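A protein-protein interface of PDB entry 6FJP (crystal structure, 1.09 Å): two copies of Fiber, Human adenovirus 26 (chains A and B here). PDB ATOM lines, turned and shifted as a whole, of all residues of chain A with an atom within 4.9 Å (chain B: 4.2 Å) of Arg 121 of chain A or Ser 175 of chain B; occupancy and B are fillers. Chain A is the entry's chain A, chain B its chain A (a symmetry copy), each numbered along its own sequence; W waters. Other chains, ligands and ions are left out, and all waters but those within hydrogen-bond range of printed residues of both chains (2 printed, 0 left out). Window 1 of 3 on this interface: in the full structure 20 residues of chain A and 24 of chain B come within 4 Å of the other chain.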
ATOM      1  N   THR A 106      -0.723  17.933 -16.777  1.00  0.00           N
ATOM      2  CA  THR A 106      -0.409  16.504 -16.831  1.00  0.00           C
ATOM      3  C   THR A 106      -1.563  15.699 -17.404  1.00  0.00           C
ATOM      4  O   THR A 106      -1.393  14.837 -18.289  1.00  0.00           O
ATOM      5  CB  THR A 106      -0.024  15.989 -15.449  1.00  0.00           C
ATOM      6  OG1 THR A 106       1.091  16.750 -14.970  1.00  0.00           O
ATOM      7  CG2 THR A 106       0.359  14.537 -15.467  1.00  0.00           C
ATOM      8  N   ALA A 107      -2.782  16.014 -16.971  1.00  0.00           N
ATOM      9  CA  ALA A 107      -3.949  15.385 -17.554  1.00  0.00           C
ATOM     10  C   ALA A 107      -4.077  15.742 -19.045  1.00  0.00           C
ATOM     11  O   ALA A 107      -4.469  14.908 -19.882  1.00  0.00           O
ATOM     12  CB  ALA A 107      -5.172  15.833 -16.796  1.00  0.00           C
ATOM     13  N   TYR A 108      -3.823  17.007 -19.338  1.00  0.00           N
ATOM     14  CA  TYR A 108      -4.135  17.577 -20.655  1.00  0.00           C
ATOM     15  C   TYR A 108      -2.880  18.273 -21.172  1.00  0.00           C
ATOM     16  O   TYR A 108      -2.710  19.494 -21.097  1.00  0.00           O
ATOM     17  CB  TYR A 108      -5.307  18.552 -20.589  1.00  0.00           C
ATOM     18  CG  TYR A 108      -6.446  18.111 -19.712  1.00  0.00           C
ATOM     19  CD1 TYR A 108      -7.145  16.927 -19.955  1.00  0.00           C
ATOM     20  CD2 TYR A 108      -6.849  18.874 -18.628  1.00  0.00           C
ATOM     21  CE1 TYR A 108      -8.203  16.550 -19.167  1.00  0.00           C
ATOM     22  CE2 TYR A 108      -7.903  18.500 -17.815  1.00  0.00           C
ATOM     23  CZ  TYR A 108      -8.593  17.333 -18.082  1.00  0.00           C
ATOM     24  OH  TYR A 108      -9.627  17.000 -17.257  1.00  0.00           O
ATOM     25  N   TYR A 119      -3.962  12.366 -26.948  1.00  0.00           N
ATOM     26  CA  TYR A 119      -4.797  11.725 -25.833  1.00  0.00           C
ATOM     27  C   TYR A 119      -6.224  12.150 -25.831  1.00  0.00           C
ATOM     28  O   TYR A 119      -6.502  13.342 -25.728  1.00  0.00           O
ATOM     29  CB  TYR A 119      -4.189  12.032 -24.481  1.00  0.00           C
ATOM     30  CG  TYR A 119      -2.847  11.382 -24.278  1.00  0.00           C
ATOM     31  CD1 TYR A 119      -2.760  10.026 -24.024  1.00  0.00           C
ATOM     32  CD2 TYR A 119      -1.645  12.072 -24.371  1.00  0.00           C
ATOM     33  CE1 TYR A 119      -1.577   9.375 -23.826  1.00  0.00           C
ATOM     34  CE2 TYR A 119      -0.421  11.417 -24.185  1.00  0.00           C
ATOM     35  CZ  TYR A 119      -0.408  10.059 -23.891  1.00  0.00           C
ATOM     36  OH  TYR A 119       0.747   9.342 -23.693  1.00  0.00           O
ATOM     37  N   SER A 120      -7.139  11.211 -25.986  1.00  0.00           N
ATOM     38  CA  SER A 120      -8.518  11.568 -26.144  1.00  0.00           C
ATOM     39  C   SER A 120      -9.134  12.225 -24.907  1.00  0.00           C
ATOM     40  O   SER A 120     -10.103  12.923 -25.036  1.00  0.00           O
ATOM     41  CB  SER A 120      -9.345  10.347 -26.568  1.00  0.00           C
ATOM     42  OG  SER A 120      -8.829   9.766 -27.729  1.00  0.00           O
ATOM     43  N   ARG A 121      -8.537  11.960 -23.734  1.00  0.00           N
ATOM     44  CA  ARG A 121      -9.107  12.538 -22.508  1.00  0.00           C
ATOM     45  C   ARG A 121      -8.984  14.064 -22.478  1.00  0.00           C
ATOM     46  O   ARG A 121      -9.659  14.723 -21.674  1.00  0.00           O
ATOM     47  CB  ARG A 121      -8.470  11.937 -21.271  1.00  0.00           C
ATOM     48  CG  ARG A 121      -7.035  12.399 -21.031  1.00  0.00           C
ATOM     49  CD  ARG A 121      -6.415  11.664 -19.870  1.00  0.00           C
ATOM     50  NE  ARG A 121      -5.069  12.192 -19.624  1.00  0.00           N
ATOM     51  CZ  ARG A 121      -4.140  11.641 -18.876  1.00  0.00           C
ATOM     52  NH1 ARG A 121      -4.363  10.548 -18.133  1.00  0.00           N
ATOM     53  NH2 ARG A 121      -2.951  12.202 -18.859  1.00  0.00           N
ATOM     54  N   THR A 122      -8.196  14.656 -23.377  1.00  0.00           N
ATOM     55  CA  THR A 122      -8.098  16.100 -23.532  1.00  0.00           C
ATOM     56  C   THR A 122      -9.363  16.727 -24.112  1.00  0.00           C
ATOM     57  O   THR A 122      -9.411  17.977 -24.170  1.00  0.00           O
ATOM     58  CB  THR A 122      -6.881  16.518 -24.372  1.00  0.00           C
ATOM     59  OG1 THR A 122      -7.049  16.060 -25.701  1.00  0.00           O
ATOM     60  CG2 THR A 122      -5.563  16.020 -23.794  1.00  0.00           C
ATOM     61  N   LYS A 123     -10.300  15.925 -24.579  1.00  0.00           N
ATOM     62  CA  LYS A 123     -11.539  16.426 -25.119  1.00  0.00           C
ATOM     63  C   LYS A 123     -12.734  15.844 -24.418  1.00  0.00           C
ATOM     64  O   LYS A 123     -12.709  14.733 -23.866  1.00  0.00           O
ATOM     65  CB  LYS A 123     -11.635  16.114 -26.602  1.00  0.00           C
ATOM     66  CG  LYS A 123     -10.692  16.981 -27.403  1.00  0.00           C
ATOM     67  CD  LYS A 123     -10.599  16.662 -28.838  1.00  0.00           C
ATOM     68  CE  LYS A 123      -9.794  17.662 -29.617  1.00  0.00           C
ATOM     69  NZ  LYS A 123      -9.790  17.335 -31.079  1.00  0.00           N
ATOM     70  N   ILE A 124     -13.820  16.633 -24.451  1.00  0.00           N
ATOM     71  CA  ILE A 124     -15.183  16.193 -24.113  1.00  0.00           C
ATOM     72  C   ILE A 124     -15.993  16.372 -25.367  1.00  0.00           C
ATOM     73  O   ILE A 124     -15.921  17.466 -25.983  1.00  0.00           O
ATOM     74  CB  ILE A 124     -15.794  17.071 -23.000  1.00  0.00           C
ATOM     75  CG1 ILE A 124     -14.951  17.004 -21.730  1.00  0.00           C
ATOM     76  CG2 ILE A 124     -17.234  16.679 -22.767  1.00  0.00           C
ATOM     77  CD1 ILE A 124     -15.231  18.220 -20.826  1.00  0.00           C
ATOM     78  N   PRO B   8      -3.166  12.097 -12.621  1.00  0.00           N
ATOM     79  CA  PRO B   8      -3.449  12.393 -14.037  1.00  0.00           C
ATOM     80  C   PRO B   8      -2.381  11.942 -15.046  1.00  0.00           C
ATOM     81  O   PRO B   8      -2.380  12.414 -16.179  1.00  0.00           O
ATOM     82  CB  PRO B   8      -3.520  13.921 -14.002  1.00  0.00           C
ATOM     83  CG  PRO B   8      -2.541  14.356 -12.975  1.00  0.00           C
ATOM     84  CD  PRO B   8      -2.700  13.309 -11.898  1.00  0.00           C
ATOM     85  N   ASP B   9      -1.446  11.070 -14.665  1.00  0.00           N
ATOM     86  CA  ASP B   9      -0.397  10.618 -15.594  1.00  0.00           C
ATOM     87  C   ASP B   9      -0.978   9.528 -16.499  1.00  0.00           C
ATOM     88  O   ASP B   9      -2.197   9.307 -16.496  1.00  0.00           O
ATOM     89  CB  ASP B   9       0.847  10.190 -14.815  1.00  0.00           C
ATOM     90  CG  ASP B   9       0.664   8.887 -14.027  1.00  0.00           C
ATOM     91  OD1 ASP B   9      -0.316   8.173 -14.229  1.00  0.00           O
ATOM     92  OD2 ASP B   9       1.567   8.557 -13.199  1.00  0.00           O
ATOM     93  N   THR B  10      -0.115   8.884 -17.302  1.00  0.00           N
ATOM     94  CA  THR B  10      -0.559   7.808 -18.169  1.00  0.00           C
ATOM     95  C   THR B  10       0.046   6.443 -17.767  1.00  0.00           C
ATOM     96  O   THR B  10       0.095   5.505 -18.606  1.00  0.00           O
ATOM     97  CB  THR B  10      -0.298   8.122 -19.666  1.00  0.00           C
ATOM     98  OG1 THR B  10       1.076   8.385 -19.893  1.00  0.00           O
ATOM     99  CG2 THR B  10      -1.221   9.289 -20.123  1.00  0.00           C
ATOM    100  N   THR B  25      -8.235   7.073 -15.991  1.00  0.00           N
ATOM    101  CA  THR B  25      -8.102   8.366 -15.375  1.00  0.00           C
ATOM    102  C   THR B  25      -9.412   8.661 -14.649  1.00  0.00           C
ATOM    103  O   THR B  25     -10.447   8.801 -15.293  1.00  0.00           O
ATOM    104  CB  THR B  25      -7.751   9.491 -16.378  1.00  0.00           C
ATOM    105  OG1 THR B  25      -6.619   9.132 -17.138  1.00  0.00           O
ATOM    106  CG2 THR B  25      -7.474  10.796 -15.680  1.00  0.00           C
ATOM    107  N   VAL B  39     -14.087  10.837 -15.684  1.00  0.00           N
ATOM    108  CA  VAL B  39     -13.449   9.560 -16.024  1.00  0.00           C
ATOM    109  C   VAL B  39     -13.076   9.492 -17.491  1.00  0.00           C
ATOM    110  O   VAL B  39     -13.824  10.010 -18.382  1.00  0.00           O
ATOM    111  CB  VAL B  39     -14.374   8.383 -15.646  1.00  0.00           C
ATOM    112  CG1 VAL B  39     -15.671   8.363 -16.433  1.00  0.00           C
ATOM    113  CG2 VAL B  39     -13.669   7.035 -15.738  1.00  0.00           C
ATOM    114  N   SER B  40     -11.993   8.775 -17.764  1.00  0.00           N
ATOM    115  CA  SER B  40     -11.675   8.335 -19.126  1.00  0.00           C
ATOM    116  C   SER B  40     -10.807   7.084 -19.012  1.00  0.00           C
ATOM    117  O   SER B  40     -10.373   6.705 -17.906  1.00  0.00           O
ATOM    118  CB  SER B  40     -10.924   9.442 -19.841  1.00  0.00           C
ATOM    119  OG  SER B  40      -9.710   9.757 -19.176  1.00  0.00           O
ATOM    120  N   VAL B 173     -10.804   7.099 -25.053  1.00  0.00           N
ATOM    121  CA  VAL B 173     -12.097   7.819 -25.121  1.00  0.00           C
ATOM    122  C   VAL B 173     -11.988   9.206 -24.504  1.00  0.00           C
ATOM    123  O   VAL B 173     -11.121   9.492 -23.650  1.00  0.00           O
ATOM    124  CB  VAL B 173     -13.213   7.029 -24.463  1.00  0.00           C
ATOM    125  CG1 VAL B 173     -13.582   5.787 -25.247  1.00  0.00           C
ATOM    126  CG2 VAL B 173     -12.900   6.675 -23.004  1.00  0.00           C
ATOM    127  N   THR B 174     -12.870  10.077 -24.967  1.00  0.00           N
ATOM    128  CA  THR B 174     -13.059  11.373 -24.376  1.00  0.00           C
ATOM    129  C   THR B 174     -13.441  11.285 -22.906  1.00  0.00           C
ATOM    130  O   THR B 174     -13.887  10.236 -22.421  1.00  0.00           O
ATOM    131  CB  THR B 174     -14.106  12.159 -25.179  1.00  0.00           C
ATOM    132  OG1 THR B 174     -15.320  11.403 -25.289  1.00  0.00           O
ATOM    133  CG2 THR B 174     -13.607  12.502 -26.551  1.00  0.00           C
ATOM    134  N   SER B 175     -13.230  12.385 -22.187  1.00  0.00           N
ATOM    135  CA  SER B 175     -13.579  12.451 -20.793  1.00  0.00           C
ATOM    136  C   SER B 175     -15.050  12.610 -20.553  1.00  0.00           C
ATOM    137  O   SER B 175     -15.759  13.278 -21.340  1.00  0.00           O
ATOM    138  CB  SER B 175     -12.836  13.619 -20.138  1.00  0.00           C
ATOM    139  OG  SER B 175     -11.424  13.359 -20.065  1.00  0.00           O
ATOM    140  N   PHE B 176     -15.538  12.064 -19.436  1.00  0.00           N
ATOM    141  CA  PHE B 176     -16.949  12.108 -19.088  1.00  0.00           C
ATOM    142  C   PHE B 176     -17.135  12.582 -17.654  1.00  0.00           C
ATOM    143  O   PHE B 176     -16.523  12.018 -16.737  1.00  0.00           O
ATOM    144  CB  PHE B 176     -17.556  10.725 -19.269  1.00  0.00           C
ATOM    145  CG  PHE B 176     -19.053  10.703 -19.110  1.00  0.00           C
ATOM    146  CD1 PHE B 176     -19.881  11.287 -20.031  1.00  0.00           C
ATOM    147  CD2 PHE B 176     -19.642  10.139 -17.998  1.00  0.00           C
ATOM    148  CE1 PHE B 176     -21.247  11.289 -19.876  1.00  0.00           C
ATOM    149  CE2 PHE B 176     -21.034  10.145 -17.824  1.00  0.00           C
ATOM    150  CZ  PHE B 176     -21.803  10.727 -18.755  1.00  0.00           C
HETATM  151  O   HOH W   1     -10.302  14.444 -17.739  1.00  0.00           O
HETATM  152  O   HOH W   2     -11.301  16.626 -20.703  1.00  0.00           O
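The guanidinium group (NH2) of Arg 121 of chain A is in hydrogen-bond range of the backbone carbonyl oxygen (O) of Pro 8 of chain B (2.7 Å). NH1 of Arg 121 of chain A sits at hydrogen-bond distance from O of Asp 9 of chain B, at 3.0 Å. OG of Ser 175 of chain B sits at hydrogen-bond distance from O of Arg 121 of chain A (2.8 Å). NH1 of Arg 121 of chain A sits at hydrogen-bond distance from OG1 of Thr 25 of chain B, at 2.8 Å. O of Lys 123 of chain A is in hydrogen-bond range of N of Ser 175 of chain B (2.9 Å). The backbone carbonyl oxygen (O) of Thr 106 of chain A sits close to the backbone carbonyl oxygen (O) of Pro 8 of chain B (3.4 Å).
Water W1 bridges OH of Tyr 108 of chain A (2.7 Å) and OG of Ser 175 of chain B (2.8 Å). Water W2 bridges O of Arg 121 of chain A (2.7 Å) and OG of Ser 175 of chain B (3.3 Å).
Of the printed residues of chain B, Arg 121 of chain A touches Pro 8 (2.7 Å), Asp 9 (3.0 Å), Thr 10 (3.6 Å), Thr 25 (2.8 Å), Ser 40 (3.3 Å), Val 173 (3.6 Å) and Ser 175 (2.8 Å). Of chain A, only Arg 121, Lys 123 and Ile 124 come within 4 Å of Ser 175 of chain B. Of the printed residues of chain B, Tyr 119 of chain A touches Thr 10 (3.7 Å). Printed residues of chain B within 4 Å of Lys 123 of chain A: Thr 174 and Ser 175. Of the printed residues of chain B, Thr 106 of chain A touches Pro 8 (3.4 Å) and Asp 9 (3.99 Å). Printed residues of chain A within 4 Å of Thr 174 of chain B: Ser 120 (3.4 Å) and Lys 123 (3.2 Å). Tyr 108 of chain A touches none of the printed residues of chain B. Thr 122 of chain A touches none of the printed residues of chain B. The nearest printed residue of chain B that does not touch Arg 121 of chain A is Thr 174 of chain B (4.5 Å). The nearest residue of chain A that does not touch Ser 175 of chain B is Ser 120 of chain A (4.3 Å).
Hydrophobic or aromatic side chains of chain A that line the printed part of chain B: Ala 107, Tyr 119 and Ile 124.
Among the printed residues, pairs that only touch across the chains: Thr 106 of chain A with Asp 9 of chain B, Ala 107 of chain A with Pro 8 of chain B, Tyr 119 of chain A with Thr 10 of chain B, Ser 120 of chain A with Val 173 of chain B, Ser 120 of chain A with Thr 174 of chain B, Arg 121 of chain A with Thr 10 of chain B, Arg 121 of chain A with Ser 40 of chain B, Arg 121 of chain A with Val 173 of chain B, Lys 123 of chain A with Thr 174 of chain B and Ile 124 of chain A with Ser 175 of chain B.
The side-chain hydroxyl (OG1) of Thr 122 of chain A lies within hydrogen-bond range of the backbone carbonyl oxygen (O) of Tyr 119 of chain A, 2.8 Å away. O of Thr 106 of chain A is in hydrogen-bond range of NH2 of Arg 121 of chain A, at 3.1 Å. N of Thr 25 of chain B sits at hydrogen-bond distance from O of Ser 40 of chain B, 2.9 Å away. The guanidinium group (NE) of Arg 121 of chain A lies within hydrogen-bond range of the backbone carbonyl oxygen (O) of Ala 107 of chain A, at 2.8 Å.
No position is printed for both chains. Of the 16 pairs that touch across the chains among the printed residues, none has its exchanged pair printed and touching as well.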
